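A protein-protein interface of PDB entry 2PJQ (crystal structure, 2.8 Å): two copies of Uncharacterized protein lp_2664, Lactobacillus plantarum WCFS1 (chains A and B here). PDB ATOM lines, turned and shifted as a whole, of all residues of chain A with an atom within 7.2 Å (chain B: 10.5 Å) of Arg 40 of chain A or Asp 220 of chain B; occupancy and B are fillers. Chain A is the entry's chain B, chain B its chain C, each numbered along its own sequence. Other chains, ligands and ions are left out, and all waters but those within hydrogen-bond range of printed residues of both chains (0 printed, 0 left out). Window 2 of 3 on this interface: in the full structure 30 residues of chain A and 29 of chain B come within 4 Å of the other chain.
Of the 22 printed residues of chain A, 7 touch a printed residue of chain B.
Of the 11 printed residues of chain B, 3 touch a printed residue of chain A.
Hydrophobic or aromatic side chains of chain B within 4 Å of the printed part of chain A: Trp 217.
Among the printed residues, 10 pairs touch across the chains.
Among the printed residues, Asp or Glu carboxylates within 4 Å of a Lys or Arg side-chain nitrogen of the other chain: Arg 202 of chain A with Asp 220 of chain B (2.8 Å).
Trp 217 of chain B touches Asp 33 of chain A (CH2 to OD1, 3.7 Å).
Arg 37 of chain A touches Trp 217 of chain B (NH1 to CZ3, 3.4 Å).
Asp 220 of chain B touches Arg 37 of chain A (OD2 to CD, 3.2 Å).
Arg 40 of chain A touches Asp 220 of chain B.
Leu 41 of chain A touches Asp 220 of chain B.
Asp 220 of chain B touches Asp 131 of chain A.
OD2 of Asp 220 of chain B touches CD1 of Ile 136 of chain A (3.98 Å).
Arg 202 of chain A touches Glu 216 of chain B (NE to CG, 3.6 Å).
The backbone NH (N) of Ile 136 of chain A sits at hydrogen-bond distance from the side-chain carboxylate (OE1) of Glu 216 of chain B (3.2 Å).
The guanidinium group (NH2) of Arg 202 of chain A lies within salt-bridge range of the side-chain carboxylate (OD1) of Asp 220 of chain B, 2.8 Å away.
Of chain B, only Asp 220 (2.8 Å) comes within 4 Å of Arg 40 of chain A.
No residue of chain B comes within 4 Å of Asn 39 of chain A.
Of the printed residues of chain B, Leu 41 of chain A touches Asp 220 (3.7 Å).
No residue of chain B comes within 4 Å of Ala 42 of chain A.
Of the printed residues of chain B, Arg 37 of chain A touches Trp 217 and Asp 220.
Of the printed residues of chain A, Trp 217 of chain B touches Asp 33 and Arg 37.
Of the printed residues of chain B, Asp 131 of chain A touches Asp 220 (3.8 Å).
Of the printed residues of chain A, Glu 216 of chain B touches Ile 136 and Arg 202.
Phe 213 of chain B touches none of the printed residues of chain A.
The nearest residue of chain B that does not touch Arg 40 of chain A is Trp 217 of chain B (4.4 Å).
The nearest residue of chain A that does not touch Asp 220 of chain B is Leu 198 of chain A (5.1 Å).
No position is printed for both chains.
Of the 10 pairs that touch across the chains among the printed residues, none has its exchanged pair printed and touching as well.
The guanidinium group (NE) of Arg 37 of chain A is in salt-bridge range of the side-chain carboxylate (OD1) of Asp 131 of chain A (2.8 Å).
The side-chain carboxylate of Asp 131 of chain A lies within hydrogen-bond range of a ring nitrogen (ND1) of His 34 of chain A, 3.2 Å away.
NH1 of Arg 202 of chain A is in hydrogen-bond range of O of Leu 130 of chain A (2.9 Å).
The side-chain amide nitrogen of Gln 212 of chain B is in hydrogen-bond range of the side-chain carboxylate of Glu 216 of chain B (2.7 Å).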
ATOM      1  N   ARG A  32       8.672   9.262 -18.955  1.00  0.00           N
ATOM      2  CA  ARG A  32       9.434   9.531 -20.161  1.00  0.00           C
ATOM      3  C   ARG A  32       8.691   9.713 -21.489  1.00  0.00           C
ATOM      4  O   ARG A  32       9.111  10.533 -22.298  1.00  0.00           O
ATOM      5  CB  ARG A  32      10.554   8.488 -20.276  1.00  0.00           C
ATOM      6  CG  ARG A  32      11.674   8.745 -19.247  1.00  0.00           C
ATOM      7  CD  ARG A  32      12.280   7.464 -18.680  1.00  0.00           C
ATOM      8  NE  ARG A  32      13.715   7.313 -18.937  1.00  0.00           N
ATOM      9  CZ  ARG A  32      14.273   7.258 -20.150  1.00  0.00           C
ATOM     10  NH1 ARG A  32      13.529   7.352 -21.258  1.00  0.00           N
ATOM     11  NH2 ARG A  32      15.584   7.082 -20.254  1.00  0.00           N
ATOM     12  N   ASP A  33       7.599   8.985 -21.729  1.00  0.00           N
ATOM     13  CA  ASP A  33       6.861   9.161 -22.987  1.00  0.00           C
ATOM     14  C   ASP A  33       6.234  10.564 -23.035  1.00  0.00           C
ATOM     15  O   ASP A  33       6.396  11.302 -24.021  1.00  0.00           O
ATOM     16  CB  ASP A  33       5.784   8.080 -23.127  1.00  0.00           C
ATOM     17  CG  ASP A  33       6.377   6.685 -23.318  1.00  0.00           C
ATOM     18  OD1 ASP A  33       7.058   6.476 -24.337  1.00  0.00           O
ATOM     19  OD2 ASP A  33       6.169   5.795 -22.456  1.00  0.00           O
ATOM     20  N   HIS A  34       5.523  10.915 -21.961  1.00  0.00           N
ATOM     21  CA  HIS A  34       4.891  12.231 -21.809  1.00  0.00           C
ATOM     22  C   HIS A  34       5.952  13.277 -22.128  1.00  0.00           C
ATOM     23  O   HIS A  34       5.811  14.057 -23.062  1.00  0.00           O
ATOM     24  CB  HIS A  34       4.406  12.407 -20.363  1.00  0.00           C
ATOM     25  CG  HIS A  34       4.037  13.820 -19.988  1.00  0.00           C
ATOM     26  ND1 HIS A  34       2.956  14.486 -20.528  1.00  0.00           N
ATOM     27  CD2 HIS A  34       4.568  14.660 -19.062  1.00  0.00           C
ATOM     28  CE1 HIS A  34       2.837  15.666 -19.948  1.00  0.00           C
ATOM     29  NE2 HIS A  34       3.801  15.795 -19.053  1.00  0.00           N
ATOM     30  N   LEU A  35       7.027  13.253 -21.351  1.00  0.00           N
ATOM     31  CA  LEU A  35       8.148  14.173 -21.516  1.00  0.00           C
ATOM     32  C   LEU A  35       8.675  14.281 -22.936  1.00  0.00           C
ATOM     33  O   LEU A  35       9.001  15.371 -23.396  1.00  0.00           O
ATOM     34  CB  LEU A  35       9.291  13.755 -20.600  1.00  0.00           C
ATOM     35  CG  LEU A  35       8.951  13.898 -19.125  1.00  0.00           C
ATOM     36  CD1 LEU A  35      10.087  13.310 -18.290  1.00  0.00           C
ATOM     37  CD2 LEU A  35       8.693  15.373 -18.802  1.00  0.00           C
ATOM     38  N   GLN A  36       8.762  13.146 -23.621  1.00  0.00           N
ATOM     39  CA  GLN A  36       9.265  13.125 -24.986  1.00  0.00           C
ATOM     40  C   GLN A  36       8.245  13.684 -25.943  1.00  0.00           C
ATOM     41  O   GLN A  36       8.607  14.407 -26.868  1.00  0.00           O
ATOM     42  CB  GLN A  36       9.635  11.707 -25.421  1.00  0.00           C
ATOM     43  CG  GLN A  36      10.704  11.069 -24.587  1.00  0.00           C
ATOM     44  CD  GLN A  36      11.555  10.117 -25.392  1.00  0.00           C
ATOM     45  OE1 GLN A  36      12.294  10.540 -26.283  1.00  0.00           O
ATOM     46  NE2 GLN A  36      11.452   8.819 -25.093  1.00  0.00           N
ATOM     47  N   ARG A  37       6.973  13.336 -25.738  1.00  0.00           N
ATOM     48  CA  ARG A  37       5.919  13.852 -26.607  1.00  0.00           C
ATOM     49  C   ARG A  37       5.858  15.383 -26.510  1.00  0.00           C
ATOM     50  O   ARG A  37       5.808  16.088 -27.529  1.00  0.00           O
ATOM     51  CB  ARG A  37       4.563  13.281 -26.216  1.00  0.00           C
ATOM     52  CG  ARG A  37       4.209  11.972 -26.882  1.00  0.00           C
ATOM     53  CD  ARG A  37       2.736  11.715 -26.705  1.00  0.00           C
ATOM     54  NE  ARG A  37       2.384  11.608 -25.301  1.00  0.00           N
ATOM     55  CZ  ARG A  37       2.723  10.571 -24.553  1.00  0.00           C
ATOM     56  NH1 ARG A  37       3.409   9.583 -25.103  1.00  0.00           N
ATOM     57  NH2 ARG A  37       2.386  10.526 -23.265  1.00  0.00           N
ATOM     58  N   VAL A  38       5.839  15.891 -25.281  1.00  0.00           N
ATOM     59  CA  VAL A  38       5.814  17.320 -25.084  1.00  0.00           C
ATOM     60  C   VAL A  38       7.060  17.888 -25.746  1.00  0.00           C
ATOM     61  O   VAL A  38       6.976  18.815 -26.533  1.00  0.00           O
ATOM     62  CB  VAL A  38       5.826  17.706 -23.582  1.00  0.00           C
ATOM     63  CG1 VAL A  38       6.269  19.155 -23.431  1.00  0.00           C
ATOM     64  CG2 VAL A  38       4.432  17.550 -22.975  1.00  0.00           C
ATOM     65  N   ASN A  39       8.219  17.328 -25.435  1.00  0.00           N
ATOM     66  CA  ASN A  39       9.452  17.833 -26.013  1.00  0.00           C
ATOM     67  C   ASN A  39       9.299  17.997 -27.516  1.00  0.00           C
ATOM     68  O   ASN A  39       9.364  19.102 -28.043  1.00  0.00           O
ATOM     69  CB  ASN A  39      10.603  16.883 -25.734  1.00  0.00           C
ATOM     70  CG  ASN A  39      11.935  17.440 -26.181  1.00  0.00           C
ATOM     71  OD1 ASN A  39      12.460  18.368 -25.568  1.00  0.00           O
ATOM     72  ND2 ASN A  39      12.486  16.885 -27.257  1.00  0.00           N
ATOM     73  N   ARG A  40       9.094  16.881 -28.202  1.00  0.00           N
ATOM     74  CA  ARG A  40       8.925  16.874 -29.646  1.00  0.00           C
ATOM     75  C   ARG A  40       7.873  17.874 -30.140  1.00  0.00           C
ATOM     76  O   ARG A  40       7.980  18.395 -31.247  1.00  0.00           O
ATOM     77  CB  ARG A  40       8.606  15.444 -30.087  1.00  0.00           C
ATOM     78  CG  ARG A  40       7.567  15.285 -31.177  1.00  0.00           C
ATOM     79  CD  ARG A  40       7.355  13.799 -31.423  1.00  0.00           C
ATOM     80  NE  ARG A  40       7.052  13.091 -30.182  1.00  0.00           N
ATOM     81  CZ  ARG A  40       6.918  11.772 -30.075  1.00  0.00           C
ATOM     82  NH1 ARG A  40       7.056  10.991 -31.144  1.00  0.00           N
ATOM     83  NH2 ARG A  40       6.647  11.230 -28.894  1.00  0.00           N
ATOM     84  N   LEU A  41       6.865  18.145 -29.313  1.00  0.00           N
ATOM     85  CA  LEU A  41       5.811  19.115 -29.651  1.00  0.00           C
ATOM     86  C   LEU A  41       6.344  20.538 -29.470  1.00  0.00           C
ATOM     87  O   LEU A  41       6.096  21.418 -30.296  1.00  0.00           O
ATOM     88  CB  LEU A  41       4.590  18.932 -28.738  1.00  0.00           C
ATOM     89  CG  LEU A  41       3.549  17.842 -29.004  1.00  0.00           C
ATOM     90  CD1 LEU A  41       2.734  17.620 -27.740  1.00  0.00           C
ATOM     91  CD2 LEU A  41       2.644  18.246 -30.163  1.00  0.00           C
ATOM     92  N   ALA A  42       7.068  20.753 -28.372  1.00  0.00           N
ATOM     93  CA  ALA A  42       7.639  22.053 -28.058  1.00  0.00           C
ATOM     94  C   ALA A  42       8.539  22.488 -29.192  1.00  0.00           C
ATOM     95  O   ALA A  42       8.492  23.636 -29.631  1.00  0.00           O
ATOM     96  CB  ALA A  42       8.438  21.973 -26.767  1.00  0.00           C
ATOM     97  N   ARG A  43       9.351  21.552 -29.674  1.00  0.00           N
ATOM     98  CA  ARG A  43      10.296  21.841 -30.740  1.00  0.00           C
ATOM     99  C   ARG A  43       9.603  22.273 -32.022  1.00  0.00           C
ATOM    100  O   ARG A  43       9.983  23.269 -32.616  1.00  0.00           O
ATOM    101  CB  ARG A  43      11.189  20.629 -30.980  1.00  0.00           C
ATOM    102  CG  ARG A  43      12.335  20.864 -31.959  1.00  0.00           C
ATOM    103  CD  ARG A  43      13.055  19.544 -32.250  1.00  0.00           C
ATOM    104  NE  ARG A  43      13.782  19.045 -31.089  1.00  0.00           N
ATOM    105  CZ  ARG A  43      14.948  19.539 -30.684  1.00  0.00           C
ATOM    106  NH1 ARG A  43      15.512  20.536 -31.359  1.00  0.00           N
ATOM    107  NH2 ARG A  43      15.547  19.056 -29.596  1.00  0.00           N
ATOM    108  N   ARG A  44       8.581  21.556 -32.459  1.00  0.00           N
ATOM    109  CA  ARG A  44       7.916  21.983 -33.678  1.00  0.00           C
ATOM    110  C   ARG A  44       7.294  23.370 -33.494  1.00  0.00           C
ATOM    111  O   ARG A  44       7.506  24.275 -34.304  1.00  0.00           O
ATOM    112  CB  ARG A  44       6.823  21.004 -34.103  1.00  0.00           C
ATOM    113  CG  ARG A  44       6.145  21.486 -35.368  1.00  0.00           C
ATOM    114  CD  ARG A  44       4.807  20.860 -35.636  1.00  0.00           C
ATOM    115  NE  ARG A  44       4.118  21.652 -36.650  1.00  0.00           N
ATOM    116  CZ  ARG A  44       2.874  21.436 -37.071  1.00  0.00           C
ATOM    117  NH1 ARG A  44       2.153  20.440 -36.571  1.00  0.00           N
ATOM    118  NH2 ARG A  44       2.341  22.229 -37.989  1.00  0.00           N
ATOM    119  N   LEU A  45       6.527  23.521 -32.418  1.00  0.00           N
ATOM    120  CA  LEU A  45       5.850  24.777 -32.103  1.00  0.00           C
ATOM    121  C   LEU A  45       6.809  25.951 -31.958  1.00  0.00           C
ATOM    122  O   LEU A  45       6.527  27.042 -32.441  1.00  0.00           O
ATOM    123  CB  LEU A  45       5.034  24.619 -30.810  1.00  0.00           C
ATOM    124  CG  LEU A  45       3.495  24.650 -30.806  1.00  0.00           C
ATOM    125  CD1 LEU A  45       2.880  23.878 -31.980  1.00  0.00           C
ATOM    126  CD2 LEU A  45       3.030  24.063 -29.474  1.00  0.00           C
ATOM    127  N   LEU A  57      12.687  24.138 -24.676  1.00  0.00           N
ATOM    128  CA  LEU A  57      12.765  22.728 -24.331  1.00  0.00           C
ATOM    129  C   LEU A  57      13.174  22.577 -22.890  1.00  0.00           C
ATOM    130  O   LEU A  57      12.616  21.747 -22.171  1.00  0.00           O
ATOM    131  CB  LEU A  57      13.754  21.993 -25.233  1.00  0.00           C
ATOM    132  CG  LEU A  57      13.519  22.217 -26.719  1.00  0.00           C
ATOM    133  CD1 LEU A  57      14.460  21.343 -27.514  1.00  0.00           C
ATOM    134  CD2 LEU A  57      12.066  21.911 -27.055  1.00  0.00           C
ATOM    135  N   TRP A  61      11.214  20.423 -20.497  1.00  0.00           N
ATOM    136  CA  TRP A  61      11.745  19.262 -19.792  1.00  0.00           C
ATOM    137  C   TRP A  61      11.499  19.359 -18.304  1.00  0.00           C
ATOM    138  O   TRP A  61      11.143  18.376 -17.659  1.00  0.00           O
ATOM    139  CB  TRP A  61      13.262  19.147 -20.002  1.00  0.00           C
ATOM    140  CG  TRP A  61      13.712  18.653 -21.343  1.00  0.00           C
ATOM    141  CD1 TRP A  61      14.493  19.322 -22.247  1.00  0.00           C
ATOM    142  CD2 TRP A  61      13.448  17.374 -21.909  1.00  0.00           C
ATOM    143  NE1 TRP A  61      14.737  18.532 -23.350  1.00  0.00           N
ATOM    144  CE2 TRP A  61      14.104  17.328 -23.169  1.00  0.00           C
ATOM    145  CE3 TRP A  61      12.723  16.252 -21.479  1.00  0.00           C
ATOM    146  CZ2 TRP A  61      14.052  16.205 -24.000  1.00  0.00           C
ATOM    147  CZ3 TRP A  61      12.673  15.136 -22.303  1.00  0.00           C
ATOM    148  CH2 TRP A  61      13.335  15.123 -23.553  1.00  0.00           C
ATOM    149  N   ALA A 127       2.365  23.161 -25.617  1.00  0.00           N
ATOM    150  CA  ALA A 127       2.878  21.822 -25.820  1.00  0.00           C
ATOM    151  C   ALA A 127       2.370  20.895 -24.725  1.00  0.00           C
ATOM    152  O   ALA A 127       1.883  19.794 -24.997  1.00  0.00           O
ATOM    153  CB  ALA A 127       4.386  21.848 -25.820  1.00  0.00           C
ATOM    154  N   LEU A 130      -1.390  20.379 -25.013  1.00  0.00           N
ATOM    155  CA  LEU A 130      -1.649  19.626 -26.234  1.00  0.00           C
ATOM    156  C   LEU A 130      -1.575  18.123 -26.026  1.00  0.00           C
ATOM    157  O   LEU A 130      -2.117  17.368 -26.816  1.00  0.00           O
ATOM    158  CB  LEU A 130      -0.672  20.046 -27.329  1.00  0.00           C
ATOM    159  CG  LEU A 130      -1.222  21.149 -28.223  1.00  0.00           C
ATOM    160  CD1 LEU A 130      -0.204  21.480 -29.257  1.00  0.00           C
ATOM    161  CD2 LEU A 130      -2.512  20.679 -28.894  1.00  0.00           C
ATOM    162  N   ASP A 131      -0.899  17.711 -24.953  1.00  0.00           N
ATOM    163  CA  ASP A 131      -0.740  16.306 -24.605  1.00  0.00           C
ATOM    164  C   ASP A 131      -1.673  15.911 -23.469  1.00  0.00           C
ATOM    165  O   ASP A 131      -1.520  14.842 -22.884  1.00  0.00           O
ATOM    166  CB  ASP A 131       0.691  16.025 -24.174  1.00  0.00           C
ATOM    167  CG  ASP A 131       1.045  14.552 -24.285  1.00  0.00           C
ATOM    168  OD1 ASP A 131       1.024  14.021 -25.428  1.00  0.00           O
ATOM    169  OD2 ASP A 131       1.333  13.914 -23.244  1.00  0.00           O
ATOM    170  N   ILE A 136      -5.062  10.650 -26.028  1.00  0.00           N
ATOM    171  CA  ILE A 136      -3.984  10.594 -25.058  1.00  0.00           C
ATOM    172  C   ILE A 136      -4.365  11.278 -23.749  1.00  0.00           C
ATOM    173  O   ILE A 136      -4.101  10.752 -22.668  1.00  0.00           O
ATOM    174  CB  ILE A 136      -2.714  11.198 -25.628  1.00  0.00           C
ATOM    175  CG1 ILE A 136      -2.017  10.139 -26.503  1.00  0.00           C
ATOM    176  CG2 ILE A 136      -1.837  11.704 -24.502  1.00  0.00           C
ATOM    177  CD1 ILE A 136      -0.751  10.608 -27.214  1.00  0.00           C
ATOM    178  N   LEU A 198      -4.035  22.072 -34.158  1.00  0.00           N
ATOM    179  CA  LEU A 198      -3.843  20.730 -33.657  1.00  0.00           C
ATOM    180  C   LEU A 198      -4.830  20.418 -32.547  1.00  0.00           C
ATOM    181  O   LEU A 198      -5.383  19.326 -32.479  1.00  0.00           O
ATOM    182  CB  LEU A 198      -2.419  20.587 -33.154  1.00  0.00           C
ATOM    183  CG  LEU A 198      -1.967  19.140 -33.108  1.00  0.00           C
ATOM    184  CD1 LEU A 198      -2.334  18.490 -34.422  1.00  0.00           C
ATOM    185  CD2 LEU A 198      -0.470  19.064 -32.844  1.00  0.00           C
ATOM    186  N   ARG A 202      -8.567  17.267 -31.545  1.00  0.00           N
ATOM    187  CA  ARG A 202      -8.323  16.528 -30.331  1.00  0.00           C
ATOM    188  C   ARG A 202      -9.398  16.770 -29.286  1.00  0.00           C
ATOM    189  O   ARG A 202      -9.243  16.371 -28.142  1.00  0.00           O
ATOM    190  CB  ARG A 202      -6.935  16.890 -29.792  1.00  0.00           C
ATOM    191  CG  ARG A 202      -5.820  16.530 -30.761  1.00  0.00           C
ATOM    192  CD  ARG A 202      -4.447  16.662 -30.151  1.00  0.00           C
ATOM    193  NE  ARG A 202      -3.458  15.966 -30.967  1.00  0.00           N
ATOM    194  CZ  ARG A 202      -2.176  15.821 -30.642  1.00  0.00           C
ATOM    195  NH1 ARG A 202      -1.715  16.335 -29.515  1.00  0.00           N
ATOM    196  NH2 ARG A 202      -1.359  15.132 -31.427  1.00  0.00           N
ATOM    197  N   TYR B 153       1.149   2.367 -22.982  1.00  0.00           N
ATOM    198  CA  TYR B 153       1.323   1.955 -24.357  1.00  0.00           C
ATOM    199  C   TYR B 153       2.776   1.945 -24.722  1.00  0.00           C
ATOM    200  O   TYR B 153       3.575   2.591 -24.077  1.00  0.00           O
ATOM    201  CB  TYR B 153       0.549   2.911 -25.256  1.00  0.00           C
ATOM    202  CG  TYR B 153       0.691   2.650 -26.731  1.00  0.00           C
ATOM    203  CD1 TYR B 153       0.368   1.406 -27.273  1.00  0.00           C
ATOM    204  CD2 TYR B 153       1.083   3.675 -27.600  1.00  0.00           C
ATOM    205  CE1 TYR B 153       0.419   1.192 -28.646  1.00  0.00           C
ATOM    206  CE2 TYR B 153       1.136   3.471 -28.967  1.00  0.00           C
ATOM    207  CZ  TYR B 153       0.793   2.226 -29.491  1.00  0.00           C
ATOM    208  OH  TYR B 153       0.752   2.042 -30.862  1.00  0.00           O
ATOM    209  N   PRO B 155       4.760   1.451 -28.607  1.00  0.00           N
ATOM    210  CA  PRO B 155       4.731   0.944 -29.980  1.00  0.00           C
ATOM    211  C   PRO B 155       5.738  -0.184 -30.199  1.00  0.00           C
ATOM    212  O   PRO B 155       5.830  -0.726 -31.296  1.00  0.00           O
ATOM    213  CB  PRO B 155       5.051   2.189 -30.805  1.00  0.00           C
ATOM    214  CG  PRO B 155       5.966   2.961 -29.888  1.00  0.00           C
ATOM    215  CD  PRO B 155       5.269   2.832 -28.556  1.00  0.00           C
ATOM    216  N   GLN B 212      -7.749   6.699 -32.442  1.00  0.00           N
ATOM    217  CA  GLN B 212      -7.505   8.098 -32.143  1.00  0.00           C
ATOM    218  C   GLN B 212      -6.212   8.212 -31.353  1.00  0.00           C
ATOM    219  O   GLN B 212      -5.380   9.085 -31.617  1.00  0.00           O
ATOM    220  CB  GLN B 212      -8.660   8.666 -31.321  1.00  0.00           C
ATOM    221  CG  GLN B 212      -9.702   9.375 -32.158  1.00  0.00           C
ATOM    222  CD  GLN B 212      -9.143  10.613 -32.812  1.00  0.00           C
ATOM    223  OE1 GLN B 212      -9.438  10.893 -33.970  1.00  0.00           O
ATOM    224  NE2 GLN B 212      -8.330  11.368 -32.069  1.00  0.00           N
ATOM    225  N   PHE B 213      -6.050   7.318 -30.381  1.00  0.00           N
ATOM    226  CA  PHE B 213      -4.857   7.293 -29.536  1.00  0.00           C
ATOM    227  C   PHE B 213      -3.570   7.120 -30.344  1.00  0.00           C
ATOM    228  O   PHE B 213      -2.636   7.903 -30.194  1.00  0.00           O
ATOM    229  CB  PHE B 213      -4.968   6.168 -28.490  1.00  0.00           C
ATOM    230  CG  PHE B 213      -3.852   6.160 -27.487  1.00  0.00           C
ATOM    231  CD1 PHE B 213      -2.540   5.906 -27.878  1.00  0.00           C
ATOM    232  CD2 PHE B 213      -4.105   6.447 -26.154  1.00  0.00           C
ATOM    233  CE1 PHE B 213      -1.500   5.943 -26.956  1.00  0.00           C
ATOM    234  CE2 PHE B 213      -3.065   6.487 -25.218  1.00  0.00           C
ATOM    235  CZ  PHE B 213      -1.762   6.234 -25.620  1.00  0.00           C
ATOM    236  N   LYS B 214      -3.529   6.102 -31.202  1.00  0.00           N
ATOM    237  CA  LYS B 214      -2.345   5.825 -32.000  1.00  0.00           C
ATOM    238  C   LYS B 214      -2.090   6.874 -33.070  1.00  0.00           C
ATOM    239  O   LYS B 214      -0.932   7.191 -33.388  1.00  0.00           O
ATOM    240  CB  LYS B 214      -2.471   4.444 -32.607  1.00  0.00           C
ATOM    241  CG  LYS B 214      -3.032   3.460 -31.594  1.00  0.00           C
ATOM    242  CD  LYS B 214      -2.262   2.149 -31.547  1.00  0.00           C
ATOM    243  CE  LYS B 214      -2.458   1.345 -32.802  1.00  0.00           C
ATOM    244  NZ  LYS B 214      -3.079   0.067 -32.440  1.00  0.00           N
ATOM    245  N   ALA B 215      -3.162   7.432 -33.624  1.00  0.00           N
ATOM    246  CA  ALA B 215      -2.998   8.473 -34.630  1.00  0.00           C
ATOM    247  C   ALA B 215      -2.270   9.621 -33.935  1.00  0.00           C
ATOM    248  O   ALA B 215      -1.200  10.045 -34.374  1.00  0.00           O
ATOM    249  CB  ALA B 215      -4.341   8.938 -35.136  1.00  0.00           C
ATOM    250  N   GLU B 216      -2.852  10.096 -32.835  1.00  0.00           N
ATOM    251  CA  GLU B 216      -2.275  11.188 -32.061  1.00  0.00           C
ATOM    252  C   GLU B 216      -0.825  10.911 -31.696  1.00  0.00           C
ATOM    253  O   GLU B 216       0.051  11.751 -31.889  1.00  0.00           O
ATOM    254  CB  GLU B 216      -3.103  11.422 -30.795  1.00  0.00           C
ATOM    255  CG  GLU B 216      -4.232  12.412 -31.004  1.00  0.00           C
ATOM    256  CD  GLU B 216      -5.338  12.333 -29.950  1.00  0.00           C
ATOM    257  OE1 GLU B 216      -5.013  12.280 -28.739  1.00  0.00           O
ATOM    258  OE2 GLU B 216      -6.532  12.345 -30.346  1.00  0.00           O
ATOM    259  N   TRP B 217      -0.576   9.720 -31.166  1.00  0.00           N
ATOM    260  CA  TRP B 217       0.765   9.339 -30.765  1.00  0.00           C
ATOM    261  C   TRP B 217       1.712   9.388 -31.938  1.00  0.00           C
ATOM    262  O   TRP B 217       2.812   9.905 -31.840  1.00  0.00           O
ATOM    263  CB  TRP B 217       0.751   7.930 -30.196  1.00  0.00           C
ATOM    264  CG  TRP B 217       2.091   7.432 -29.826  1.00  0.00           C
ATOM    265  CD1 TRP B 217       3.152   7.251 -30.652  1.00  0.00           C
ATOM    266  CD2 TRP B 217       2.510   7.004 -28.526  1.00  0.00           C
ATOM    267  NE1 TRP B 217       4.213   6.729 -29.950  1.00  0.00           N
ATOM    268  CE2 TRP B 217       3.844   6.568 -28.640  1.00  0.00           C
ATOM    269  CE3 TRP B 217       1.885   6.943 -27.275  1.00  0.00           C
ATOM    270  CZ2 TRP B 217       4.569   6.082 -27.553  1.00  0.00           C
ATOM    271  CZ3 TRP B 217       2.612   6.453 -26.190  1.00  0.00           C
ATOM    272  CH2 TRP B 217       3.937   6.032 -26.339  1.00  0.00           C
ATOM    273  N   THR B 218       1.287   8.823 -33.055  1.00  0.00           N
ATOM    274  CA  THR B 218       2.137   8.819 -34.232  1.00  0.00           C
ATOM    275  C   THR B 218       2.384  10.233 -34.744  1.00  0.00           C
ATOM    276  O   THR B 218       3.492  10.566 -35.148  1.00  0.00           O
ATOM    277  CB  THR B 218       1.524   7.954 -35.325  1.00  0.00           C
ATOM    278  OG1 THR B 218       1.530   6.588 -34.889  1.00  0.00           O
ATOM    279  CG2 THR B 218       2.311   8.089 -36.611  1.00  0.00           C
ATOM    280  N   ALA B 219       1.351  11.065 -34.716  1.00  0.00           N
ATOM    281  CA  ALA B 219       1.481  12.441 -35.153  1.00  0.00           C
ATOM    282  C   ALA B 219       2.574  13.104 -34.332  1.00  0.00           C
ATOM    283  O   ALA B 219       3.531  13.636 -34.891  1.00  0.00           O
ATOM    284  CB  ALA B 219       0.172  13.178 -34.963  1.00  0.00           C
ATOM    285  N   ASP B 220       2.441  13.065 -33.005  1.00  0.00           N
ATOM    286  CA  ASP B 220       3.439  13.682 -32.155  1.00  0.00           C
ATOM    287  C   ASP B 220       4.765  13.138 -32.568  1.00  0.00           C
ATOM    288  O   ASP B 220       5.393  13.748 -33.452  1.00  0.00           O
ATOM    289  CB  ASP B 220       3.214  13.350 -30.692  1.00  0.00           C
ATOM    290  CG  ASP B 220       1.894  13.854 -30.181  1.00  0.00           C
ATOM    291  OD1 ASP B 220       1.338  14.793 -30.797  1.00  0.00           O
ATOM    292  OD2 ASP B 220       1.421  13.317 -29.157  1.00  0.00           O
